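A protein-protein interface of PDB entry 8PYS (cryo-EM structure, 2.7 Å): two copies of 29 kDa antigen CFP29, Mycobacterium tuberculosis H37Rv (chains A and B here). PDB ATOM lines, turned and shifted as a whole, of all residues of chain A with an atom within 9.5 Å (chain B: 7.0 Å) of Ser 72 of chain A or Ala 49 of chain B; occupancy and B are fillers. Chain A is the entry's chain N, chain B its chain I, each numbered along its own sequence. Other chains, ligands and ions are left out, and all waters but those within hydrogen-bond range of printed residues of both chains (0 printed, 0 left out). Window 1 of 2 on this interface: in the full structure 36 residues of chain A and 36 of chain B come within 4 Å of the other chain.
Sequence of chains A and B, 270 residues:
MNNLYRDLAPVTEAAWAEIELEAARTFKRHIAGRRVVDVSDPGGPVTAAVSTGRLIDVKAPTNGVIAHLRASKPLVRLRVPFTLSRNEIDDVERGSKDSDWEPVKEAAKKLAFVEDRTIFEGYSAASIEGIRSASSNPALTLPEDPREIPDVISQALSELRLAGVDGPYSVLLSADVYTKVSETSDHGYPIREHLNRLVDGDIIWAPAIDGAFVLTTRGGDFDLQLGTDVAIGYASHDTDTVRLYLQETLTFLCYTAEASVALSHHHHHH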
ATOM      1  N   VAL A  46      12.514 -21.261  -8.201  1.00  0.00           N
ATOM      2  CA  VAL A  46      11.344 -21.432  -9.057  1.00  0.00           C
ATOM      3  C   VAL A  46      11.754 -21.561 -10.520  1.00  0.00           C
ATOM      4  O   VAL A  46      11.137 -22.311 -11.285  1.00  0.00           O
ATOM      5  CB  VAL A  46      10.354 -20.275  -8.847  1.00  0.00           C
ATOM      6  CG1 VAL A  46       9.029 -20.585  -9.524  1.00  0.00           C
ATOM      7  CG2 VAL A  46      10.153 -20.018  -7.368  1.00  0.00           C
ATOM      8  N   THR A  47      12.786 -20.827 -10.933  1.00  0.00           N
ATOM      9  CA  THR A  47      13.181 -20.774 -12.336  1.00  0.00           C
ATOM     10  C   THR A  47      13.508 -22.160 -12.874  1.00  0.00           C
ATOM     11  O   THR A  47      14.327 -22.886 -12.308  1.00  0.00           O
ATOM     12  CB  THR A  47      14.388 -19.848 -12.498  1.00  0.00           C
ATOM     13  OG1 THR A  47      14.037 -18.526 -12.073  1.00  0.00           O
ATOM     14  CG2 THR A  47      14.846 -19.808 -13.944  1.00  0.00           C
ATOM     15  N   ALA A  48      12.869 -22.513 -13.992  1.00  0.00           N
ATOM     16  CA  ALA A  48      13.020 -23.827 -14.597  1.00  0.00           C
ATOM     17  C   ALA A  48      13.464 -23.797 -16.049  1.00  0.00           C
ATOM     18  O   ALA A  48      13.886 -24.836 -16.563  1.00  0.00           O
ATOM     19  CB  ALA A  48      11.702 -24.613 -14.512  1.00  0.00           C
ATOM     20  N   ALA A  49      13.382 -22.654 -16.722  1.00  0.00           N
ATOM     21  CA  ALA A  49      13.771 -22.582 -18.124  1.00  0.00           C
ATOM     22  C   ALA A  49      14.185 -21.159 -18.456  1.00  0.00           C
ATOM     23  O   ALA A  49      13.866 -20.213 -17.732  1.00  0.00           O
ATOM     24  CB  ALA A  49      12.638 -23.043 -19.045  1.00  0.00           C
ATOM     25  N   VAL A  50      14.911 -21.025 -19.561  1.00  0.00           N
ATOM     26  CA  VAL A  50      15.345 -19.734 -20.077  1.00  0.00           C
ATOM     27  C   VAL A  50      14.782 -19.581 -21.480  1.00  0.00           C
ATOM     28  O   VAL A  50      14.971 -20.458 -22.329  1.00  0.00           O
ATOM     29  CB  VAL A  50      16.880 -19.608 -20.082  1.00  0.00           C
ATOM     30  CG1 VAL A  50      17.309 -18.338 -20.796  1.00  0.00           C
ATOM     31  CG2 VAL A  50      17.409 -19.626 -18.663  1.00  0.00           C
ATOM     32  N   SER A  51      14.088 -18.474 -21.719  1.00  0.00           N
ATOM     33  CA  SER A  51      13.462 -18.250 -23.014  1.00  0.00           C
ATOM     34  C   SER A  51      14.517 -17.926 -24.061  1.00  0.00           C
ATOM     35  O   SER A  51      15.376 -17.065 -23.848  1.00  0.00           O
ATOM     36  CB  SER A  51      12.443 -17.118 -22.913  1.00  0.00           C
ATOM     37  OG  SER A  51      12.008 -16.705 -24.195  1.00  0.00           O
ATOM     38  N   THR A  52      14.458 -18.621 -25.193  1.00  0.00           N
ATOM     39  CA  THR A  52      15.346 -18.341 -26.309  1.00  0.00           C
ATOM     40  C   THR A  52      14.771 -17.318 -27.275  1.00  0.00           C
ATOM     41  O   THR A  52      15.461 -16.922 -28.218  1.00  0.00           O
ATOM     42  CB  THR A  52      15.675 -19.630 -27.067  1.00  0.00           C
ATOM     43  OG1 THR A  52      14.516 -20.086 -27.772  1.00  0.00           O
ATOM     44  CG2 THR A  52      16.119 -20.707 -26.102  1.00  0.00           C
ATOM     45  N   GLY A  53      13.528 -16.889 -27.066  1.00  0.00           N
ATOM     46  CA  GLY A  53      12.904 -15.887 -27.896  1.00  0.00           C
ATOM     47  C   GLY A  53      12.384 -16.379 -29.225  1.00  0.00           C
ATOM     48  O   GLY A  53      11.874 -15.571 -30.006  1.00  0.00           O
ATOM     49  N   ARG A  54      12.478 -17.673 -29.505  1.00  0.00           N
ATOM     50  CA  ARG A  54      12.106 -18.224 -30.798  1.00  0.00           C
ATOM     51  C   ARG A  54      10.783 -18.971 -30.703  1.00  0.00           C
ATOM     52  O   ARG A  54      10.242 -19.206 -29.622  1.00  0.00           O
ATOM     53  CB  ARG A  54      13.210 -19.145 -31.326  1.00  0.00           C
ATOM     54  CG  ARG A  54      14.501 -18.413 -31.623  1.00  0.00           C
ATOM     55  CD  ARG A  54      15.556 -19.339 -32.185  1.00  0.00           C
ATOM     56  NE  ARG A  54      16.838 -18.660 -32.309  1.00  0.00           N
ATOM     57  CZ  ARG A  54      17.145 -17.806 -33.277  1.00  0.00           C
ATOM     58  NH1 ARG A  54      16.288 -17.517 -34.241  1.00  0.00           N
ATOM     59  NH2 ARG A  54      18.342 -17.227 -33.277  1.00  0.00           N
ATOM     60  N   LEU A  55      10.265 -19.339 -31.870  1.00  0.00           N
ATOM     61  CA  LEU A  55       8.985 -20.012 -31.995  1.00  0.00           C
ATOM     62  C   LEU A  55       9.177 -21.360 -32.672  1.00  0.00           C
ATOM     63  O   LEU A  55      10.045 -21.525 -33.530  1.00  0.00           O
ATOM     64  CB  LEU A  55       7.991 -19.173 -32.804  1.00  0.00           C
ATOM     65  CG  LEU A  55       7.760 -17.733 -32.350  1.00  0.00           C
ATOM     66  CD1 LEU A  55       6.908 -16.995 -33.358  1.00  0.00           C
ATOM     67  CD2 LEU A  55       7.114 -17.697 -30.980  1.00  0.00           C
ATOM     68  N   ILE A  56       8.355 -22.325 -32.277  1.00  0.00           N
ATOM     69  CA  ILE A  56       8.349 -23.652 -32.877  1.00  0.00           C
ATOM     70  C   ILE A  56       6.990 -23.874 -33.519  1.00  0.00           C
ATOM     71  O   ILE A  56       5.954 -23.644 -32.885  1.00  0.00           O
ATOM     72  CB  ILE A  56       8.652 -24.751 -31.844  1.00  0.00           C
ATOM     73  CG1 ILE A  56       9.929 -24.424 -31.073  1.00  0.00           C
ATOM     74  CG2 ILE A  56       8.785 -26.094 -32.531  1.00  0.00           C
ATOM     75  CD1 ILE A  56       9.851 -24.775 -29.615  1.00  0.00           C
ATOM     76  N   LEU A  69       4.738 -22.689 -30.475  1.00  0.00           N
ATOM     77  CA  LEU A  69       5.246 -22.927 -29.134  1.00  0.00           C
ATOM     78  C   LEU A  69       6.405 -21.988 -28.834  1.00  0.00           C
ATOM     79  O   LEU A  69       7.239 -21.711 -29.698  1.00  0.00           O
ATOM     80  CB  LEU A  69       5.701 -24.375 -28.976  1.00  0.00           C
ATOM     81  CG  LEU A  69       4.630 -25.406 -28.635  1.00  0.00           C
ATOM     82  CD1 LEU A  69       5.233 -26.797 -28.618  1.00  0.00           C
ATOM     83  CD2 LEU A  69       3.984 -25.082 -27.303  1.00  0.00           C
ATOM     84  N   ARG A  70       6.450 -21.494 -27.602  1.00  0.00           N
ATOM     85  CA  ARG A  70       7.551 -20.646 -27.167  1.00  0.00           C
ATOM     86  C   ARG A  70       8.740 -21.519 -26.786  1.00  0.00           C
ATOM     87  O   ARG A  70       8.654 -22.323 -25.851  1.00  0.00           O
ATOM     88  CB  ARG A  70       7.124 -19.773 -25.992  1.00  0.00           C
ATOM     89  CG  ARG A  70       6.139 -18.686 -26.363  1.00  0.00           C
ATOM     90  CD  ARG A  70       6.740 -17.728 -27.374  1.00  0.00           C
ATOM     91  NE  ARG A  70       8.026 -17.208 -26.930  1.00  0.00           N
ATOM     92  CZ  ARG A  70       8.203 -16.018 -26.379  1.00  0.00           C
ATOM     93  NH1 ARG A  70       7.199 -15.173 -26.221  1.00  0.00           N
ATOM     94  NH2 ARG A  70       9.419 -15.664 -25.977  1.00  0.00           N
ATOM     95  N   ALA A  71       9.842 -21.366 -27.512  1.00  0.00           N
ATOM     96  CA  ALA A  71      11.035 -22.152 -27.244  1.00  0.00           C
ATOM     97  C   ALA A  71      11.725 -21.676 -25.972  1.00  0.00           C
ATOM     98  O   ALA A  71      11.714 -20.489 -25.635  1.00  0.00           O
ATOM     99  CB  ALA A  71      12.003 -22.074 -28.420  1.00  0.00           C
ATOM    100  N   SER A  72      12.327 -22.625 -25.261  1.00  0.00           N
ATOM    101  CA  SER A  72      13.079 -22.325 -24.053  1.00  0.00           C
ATOM    102  C   SER A  72      14.085 -23.440 -23.820  1.00  0.00           C
ATOM    103  O   SER A  72      13.974 -24.528 -24.389  1.00  0.00           O
ATOM    104  CB  SER A  72      12.158 -22.159 -22.839  1.00  0.00           C
ATOM    105  OG  SER A  72      11.307 -23.279 -22.683  1.00  0.00           O
ATOM    106  N   LYS A  73      15.074 -23.151 -22.979  1.00  0.00           N
ATOM    107  CA  LYS A  73      16.095 -24.127 -22.622  1.00  0.00           C
ATOM    108  C   LYS A  73      15.968 -24.480 -21.151  1.00  0.00           C
ATOM    109  O   LYS A  73      16.027 -23.583 -20.296  1.00  0.00           O
ATOM    110  CB  LYS A  73      17.489 -23.591 -22.926  1.00  0.00           C
ATOM    111  CG  LYS A  73      17.748 -23.441 -24.403  1.00  0.00           C
ATOM    112  CD  LYS A  73      18.122 -24.770 -25.024  1.00  0.00           C
ATOM    113  CE  LYS A  73      18.393 -24.622 -26.505  1.00  0.00           C
ATOM    114  NZ  LYS A  73      19.771 -24.139 -26.755  1.00  0.00           N
ATOM    115  N   PRO A  74      15.784 -25.750 -20.806  1.00  0.00           N
ATOM    116  CA  PRO A  74      15.564 -26.112 -19.403  1.00  0.00           C
ATOM    117  C   PRO A  74      16.846 -26.049 -18.589  1.00  0.00           C
ATOM    118  O   PRO A  74      17.922 -26.433 -19.052  1.00  0.00           O
ATOM    119  CB  PRO A  74      15.037 -27.548 -19.492  1.00  0.00           C
ATOM    120  CG  PRO A  74      15.646 -28.086 -20.738  1.00  0.00           C
ATOM    121  CD  PRO A  74      15.802 -26.928 -21.691  1.00  0.00           C
ATOM    122  N   LEU A  75      16.721 -25.551 -17.363  1.00  0.00           N
ATOM    123  CA  LEU A  75      17.825 -25.626 -16.422  1.00  0.00           C
ATOM    124  C   LEU A  75      17.984 -27.058 -15.933  1.00  0.00           C
ATOM    125  O   LEU A  75      17.005 -27.794 -15.792  1.00  0.00           O
ATOM    126  CB  LEU A  75      17.591 -24.700 -15.230  1.00  0.00           C
ATOM    127  CG  LEU A  75      17.308 -23.218 -15.456  1.00  0.00           C
ATOM    128  CD1 LEU A  75      17.503 -22.468 -14.161  1.00  0.00           C
ATOM    129  CD2 LEU A  75      18.187 -22.641 -16.534  1.00  0.00           C
ATOM    130  N   ALA A 126      20.746 -32.406 -21.287  1.00  0.00           N
ATOM    131  CA  ALA A 126      20.153 -31.175 -20.791  1.00  0.00           C
ATOM    132  C   ALA A 126      19.848 -30.184 -21.904  1.00  0.00           C
ATOM    133  O   ALA A 126      19.558 -29.019 -21.615  1.00  0.00           O
ATOM    134  CB  ALA A 126      21.074 -30.525 -19.756  1.00  0.00           C
ATOM    135  N   SER A 127      19.905 -30.626 -23.162  1.00  0.00           N
ATOM    136  CA  SER A 127      19.698 -29.765 -24.325  1.00  0.00           C
ATOM    137  C   SER A 127      20.673 -28.594 -24.338  1.00  0.00           C
ATOM    138  O   SER A 127      20.314 -27.474 -24.707  1.00  0.00           O
ATOM    139  CB  SER A 127      18.252 -29.261 -24.399  1.00  0.00           C
ATOM    140  OG  SER A 127      17.332 -30.329 -24.274  1.00  0.00           O
ATOM    141  N   ILE A 128      21.915 -28.842 -23.934  1.00  0.00           N
ATOM    142  CA  ILE A 128      22.952 -27.821 -23.899  1.00  0.00           C
ATOM    143  C   ILE A 128      24.002 -28.185 -24.936  1.00  0.00           C
ATOM    144  O   ILE A 128      24.581 -29.275 -24.888  1.00  0.00           O
ATOM    145  CB  ILE A 128      23.581 -27.687 -22.504  1.00  0.00           C
ATOM    146  CG1 ILE A 128      22.582 -27.059 -21.532  1.00  0.00           C
ATOM    147  CG2 ILE A 128      24.848 -26.852 -22.572  1.00  0.00           C
ATOM    148  CD1 ILE A 128      22.961 -27.201 -20.078  1.00  0.00           C
ATOM    149  N   THR A 251      21.942 -23.471 -16.842  1.00  0.00           N
ATOM    150  CA  THR A 251      22.027 -23.843 -18.243  1.00  0.00           C
ATOM    151  C   THR A 251      23.040 -22.912 -18.891  1.00  0.00           C
ATOM    152  O   THR A 251      23.344 -21.839 -18.367  1.00  0.00           O
ATOM    153  CB  THR A 251      20.664 -23.768 -18.948  1.00  0.00           C
ATOM    154  OG1 THR A 251      20.666 -24.620 -20.099  1.00  0.00           O
ATOM    155  CG2 THR A 251      20.351 -22.346 -19.383  1.00  0.00           C
ATOM    156  N   LEU A 253      24.090 -21.065 -22.619  1.00  0.00           N
ATOM    157  CA  LEU A 253      23.651 -20.683 -23.954  1.00  0.00           C
ATOM    158  C   LEU A 253      24.779 -19.963 -24.669  1.00  0.00           C
ATOM    159  O   LEU A 253      25.383 -19.039 -24.115  1.00  0.00           O
ATOM    160  CB  LEU A 253      22.412 -19.788 -23.896  1.00  0.00           C
ATOM    161  CG  LEU A 253      21.330 -20.211 -22.905  1.00  0.00           C
ATOM    162  CD1 LEU A 253      20.306 -19.111 -22.739  1.00  0.00           C
ATOM    163  CD2 LEU A 253      20.673 -21.492 -23.368  1.00  0.00           C
ATOM    164  N   VAL B  46       8.795 -11.820 -23.460  1.00  0.00           N
ATOM    165  CA  VAL B  46       9.962 -12.666 -23.235  1.00  0.00           C
ATOM    166  C   VAL B  46       9.550 -14.030 -22.694  1.00  0.00           C
ATOM    167  O   VAL B  46      10.164 -15.052 -23.025  1.00  0.00           O
ATOM    168  CB  VAL B  46      10.957 -11.964 -22.295  1.00  0.00           C
ATOM    169  CG1 VAL B  46      12.280 -12.711 -22.273  1.00  0.00           C
ATOM    170  CG2 VAL B  46      11.162 -10.526 -22.726  1.00  0.00           C
ATOM    171  N   THR B  47       8.520 -14.069 -21.850  1.00  0.00           N
ATOM    172  CA  THR B  47       8.124 -15.300 -21.175  1.00  0.00           C
ATOM    173  C   THR B  47       7.791 -16.400 -22.174  1.00  0.00           C
ATOM    174  O   THR B  47       6.971 -16.216 -23.075  1.00  0.00           O
ATOM    175  CB  THR B  47       6.919 -15.027 -20.273  1.00  0.00           C
ATOM    176  OG1 THR B  47       7.275 -14.058 -19.280  1.00  0.00           O
ATOM    177  CG2 THR B  47       6.460 -16.302 -19.589  1.00  0.00           C
ATOM    178  N   ALA B  48       8.428 -17.560 -21.993  1.00  0.00           N
ATOM    179  CA  ALA B  48       8.271 -18.687 -22.897  1.00  0.00           C
ATOM    180  C   ALA B  48       7.825 -19.972 -22.220  1.00  0.00           C
ATOM    181  O   ALA B  48       7.399 -20.895 -22.920  1.00  0.00           O
ATOM    182  CB  ALA B  48       9.587 -18.966 -23.641  1.00  0.00           C
ATOM    183  N   ALA B  49       7.910 -20.064 -20.896  1.00  0.00           N
ATOM    184  CA  ALA B  49       7.519 -21.284 -20.206  1.00  0.00           C
ATOM    185  C   ALA B  49       7.110 -20.944 -18.783  1.00  0.00           C
ATOM    186  O   ALA B  49       7.433 -19.875 -18.261  1.00  0.00           O
ATOM    187  CB  ALA B  49       8.649 -22.318 -20.209  1.00  0.00           C
ATOM    188  N   VAL B  50       6.382 -21.871 -18.168  1.00  0.00           N
ATOM    189  CA  VAL B  50       5.952 -21.755 -16.782  1.00  0.00           C
ATOM    190  C   VAL B  50       6.514 -22.943 -16.019  1.00  0.00           C
ATOM    191  O   VAL B  50       6.319 -24.094 -16.423  1.00  0.00           O
ATOM    192  CB  VAL B  50       4.416 -21.699 -16.663  1.00  0.00           C
ATOM    193  CG1 VAL B  50       3.991 -21.768 -15.206  1.00  0.00           C
ATOM    194  CG2 VAL B  50       3.889 -20.435 -17.311  1.00  0.00           C
ATOM    195  N   SER B  51       7.210 -22.664 -14.923  1.00  0.00           N
ATOM    196  CA  SER B  51       7.834 -23.724 -14.146  1.00  0.00           C
ATOM    197  C   SER B  51       6.779 -24.513 -13.385  1.00  0.00           C
ATOM    198  O   SER B  51       5.924 -23.935 -12.708  1.00  0.00           O
ATOM    199  CB  SER B  51       8.858 -23.131 -13.180  1.00  0.00           C
ATOM    200  OG  SER B  51       9.292 -24.094 -12.240  1.00  0.00           O
ATOM    201  N   SER B  72       8.953 -27.693 -17.057  1.00  0.00           N
ATOM    202  CA  SER B  72       8.203 -26.475 -17.327  1.00  0.00           C
ATOM    203  C   SER B  72       7.195 -26.763 -18.427  1.00  0.00           C
ATOM    204  O   SER B  72       7.301 -27.758 -19.146  1.00  0.00           O
ATOM    205  CB  SER B  72       9.126 -25.317 -17.724  1.00  0.00           C
ATOM    206  OG  SER B  72       9.975 -25.680 -18.796  1.00  0.00           O
ATOM    207  N   LYS B  73       6.207 -25.878 -18.542  1.00  0.00           N
ATOM    208  CA  LYS B  73       5.184 -25.992 -19.572  1.00  0.00           C
ATOM    209  C   LYS B  73       5.312 -24.833 -20.546  1.00  0.00           C
ATOM    210  O   LYS B  73       5.256 -23.669 -20.125  1.00  0.00           O
ATOM    211  CB  LYS B  73       3.791 -26.020 -18.954  1.00  0.00           C
ATOM    212  CG  LYS B  73       3.529 -27.275 -18.159  1.00  0.00           C
ATOM    213  CD  LYS B  73       3.151 -28.423 -19.069  1.00  0.00           C
ATOM    214  CE  LYS B  73       2.879 -29.681 -18.275  1.00  0.00           C
ATOM    215  NZ  LYS B  73       1.501 -29.685 -17.729  1.00  0.00           N
ATOM    216  N   PRO B  74       5.492 -25.095 -21.837  1.00  0.00           N
ATOM    217  CA  PRO B  74       5.714 -24.001 -22.788  1.00  0.00           C
ATOM    218  C   PRO B  74       4.433 -23.241 -23.092  1.00  0.00           C
ATOM    219  O   PRO B  74       3.354 -23.824 -23.227  1.00  0.00           O
ATOM    220  CB  PRO B  74       6.236 -24.725 -24.034  1.00  0.00           C
ATOM    221  CG  PRO B  74       5.622 -26.077 -23.956  1.00  0.00           C
ATOM    222  CD  PRO B  74       5.469 -26.412 -22.495  1.00  0.00           C
ATOM    223  N   LEU B  75       4.561 -21.923 -23.195  1.00  0.00           N
ATOM    224  CA  LEU B  75       3.458 -21.111 -23.680  1.00  0.00           C
ATOM    225  C   LEU B  75       3.296 -21.312 -25.180  1.00  0.00           C
ATOM    226  O   LEU B  75       4.272 -21.518 -25.903  1.00  0.00           O
ATOM    227  CB  LEU B  75       3.697 -19.632 -23.385  1.00  0.00           C
ATOM    228  CG  LEU B  75       3.984 -19.172 -21.958  1.00  0.00           C
ATOM    229  CD1 LEU B  75       3.793 -17.678 -21.866  1.00  0.00           C
ATOM    230  CD2 LEU B  75       3.106 -19.878 -20.959  1.00  0.00           C
ATOM    231  N   GLN B 225      -1.981 -19.150 -17.337  1.00  0.00           N
ATOM    232  CA  GLN B 225      -0.791 -18.312 -17.360  1.00  0.00           C
ATOM    233  C   GLN B 225      -0.711 -17.589 -18.698  1.00  0.00           C
ATOM    234  O   GLN B 225      -0.680 -18.227 -19.753  1.00  0.00           O
ATOM    235  CB  GLN B 225       0.457 -19.155 -17.119  1.00  0.00           C
ATOM    236  CG  GLN B 225       0.580 -19.674 -15.700  1.00  0.00           C
ATOM    237  CD  GLN B 225       0.950 -18.586 -14.721  1.00  0.00           C
ATOM    238  OE1 GLN B 225       0.259 -18.369 -13.726  1.00  0.00           O
ATOM    239  NE2 GLN B 225       2.043 -17.888 -14.996  1.00  0.00           N
ATOM    240  N   THR B 251      -0.653 -20.512 -21.555  1.00  0.00           N
ATOM    241  CA  THR B 251      -0.741 -21.933 -21.262  1.00  0.00           C
ATOM    242  C   THR B 251      -1.751 -22.094 -20.137  1.00  0.00           C
ATOM    243  O   THR B 251      -2.052 -21.144 -19.411  1.00  0.00           O
ATOM    244  CB  THR B 251       0.621 -22.532 -20.884  1.00  0.00           C
ATOM    245  OG1 THR B 251       0.615 -23.943 -21.131  1.00  0.00           O
ATOM    246  CG2 THR B 251       0.938 -22.286 -19.418  1.00  0.00           C
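Among the printed residues, pairs that only touch across the chains: Ala 71 of chain A with Ala 48 of chain B (3.3 Å), Ala 48 of chain A with Ser 51 of chain B (3.4 Å), Ser 51 of chain A with Ala 48 of chain B (3.4 Å), Leu 69 of chain A with Leu 75 of chain B (3.7 Å), Ala 49 of chain A with Ser 72 of chain B (3.8 Å), Ser 72 of chain A with Ala 49 of chain B (3.8 Å), Leu 69 of chain A with Pro 74 of chain B (3.9 Å) and Arg 70 of chain A with Pro 74 of chain B (3.9 Å).
Of the 23 printed residues of chain A, 8 touch a printed residue of chain B. Hydrophobic or aromatic side chains of chain A within 4 Å of the printed part of chain B: Ala 48, Ala 49 and Leu 69. Of the 12 printed residues of chain B, 8 touch a printed residue of chain A. Printed residues of chain B that touch a printed residue of chain A: Val 46, Thr 47, Ala 48, Ala 49, Ser 51, Ser 72, Pro 74 and Leu 75. Hydrophobic or aromatic side chains of chain B within 4 Å of the printed part of chain A: Ala 48, Ala 49, Pro 74 and Leu 75. Among the printed residues, no Asp or Glu carboxylate lies within 4 Å of a Lys or Arg side-chain nitrogen of the other chain.
Val 46 of chain A touches Ser 51 of chain B, and with the chains exchanged Ser 51 of chain A touches Val 46 of chain B. Ala 48 of chain A touches Ser 51 of chain B, and with the chains exchanged Ser 51 of chain A touches Ala 48 of chain B. Ala 49 of chain A touches Ser 72 of chain B, and with the chains exchanged Ser 72 of chain A touches Ala 49 of chain B. Positions printed for both chains: 46, 47, 48, 49, 50, 51, 72, 73, 74, 75 and 251. Of the 14 pairs that touch across the chains among the printed residues, 6 have their exchanged pair printed and touching as well.
Of chain B, only Ala 49 comes within 4 Å of Ser 72 of chain A. Of chain A, only Ser 72 comes within 4 Å of Ala 49 of chain B. Of chain A, only Ser 51, Arg 70 and Ala 71 come within 4 Å of Ala 48 of chain B. Val 50 of chain B touches none of the printed residues of chain A. Of the printed residues of chain A, Ser 72 of chain B touches Ala 49 (3.8 Å). Of the printed residues of chain A, Leu 75 of chain B touches Leu 69 (3.7 Å) and Arg 70 (2.8 Å). Printed residues of chain B within 4 Å of Ala 48 of chain A: Ser 51 (3.4 Å). Printed residues of chain B within 4 Å of Val 46 of chain A: Ser 51. Of the printed residues of chain B, Ser 51 of chain A touches Val 46 and Ala 48. Arg 54 of chain A touches none of the printed residues of chain B. Lys 73 of chain A touches none of the printed residues of chain B. The nearest residue of chain B that does not touch Ser 72 of chain A is Ala 48 of chain B (4.2 Å). The nearest residue of chain A that does not touch Ala 49 of chain B is Ala 49 of chain A (4.2 Å).
The side-chain hydroxyl (OG) of Ser 51 of chain A lies within hydrogen-bond range of the backbone NH (N) of Gly 53 of chain A, at 3.3 Å. OG1 of Thr 251 of chain B is in hydrogen-bond range of O of Pro 74 of chain B, 3.5 Å away. O of Ala 48 of chain B is in hydrogen-bond range of N of Leu 75 of chain B, 3.0 Å away. The backbone carbonyl oxygen (O) of Ile 56 of chain A lies within hydrogen-bond range of the backbone NH (N) of Leu 69 of chain A (2.9 Å). N of Thr 52 of chain A is in hydrogen-bond range of O of Ala 71 of chain A, 3.3 Å away. The side-chain hydroxyl (OG) of Ser 51 of chain A is in hydrogen-bond range of the guanidinium group (NH2) of Arg 70 of chain A (3.3 Å).
The side-chain hydroxyl of Ser 51 of chain B lies within hydrogen-bond range of the backbone carbonyl oxygen of Val 46 of chain A, at 2.7 Å. The backbone carbonyl oxygen (O) of Val 46 of chain B lies within hydrogen-bond range of the side-chain hydroxyl (OG) of Ser 51 of chain A (2.7 Å). O of Val 46 of chain B sits at hydrogen-bond distance from NH2 of Arg 70 of chain A, at 3.1 Å. The backbone carbonyl oxygen of Thr 47 of chain B sits at hydrogen-bond distance from the guanidinium group of Arg 70 of chain A (3.3 Å). The backbone carbonyl oxygen (O) of Arg 70 of chain A sits close to the backbone carbonyl oxygen (O) of Ala 48 of chain B (3.5 Å). The backbone carbonyl oxygen (O) of Leu 75 of chain B is in hydrogen-bond range of the backbone NH (N) of Arg 70 of chain A.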
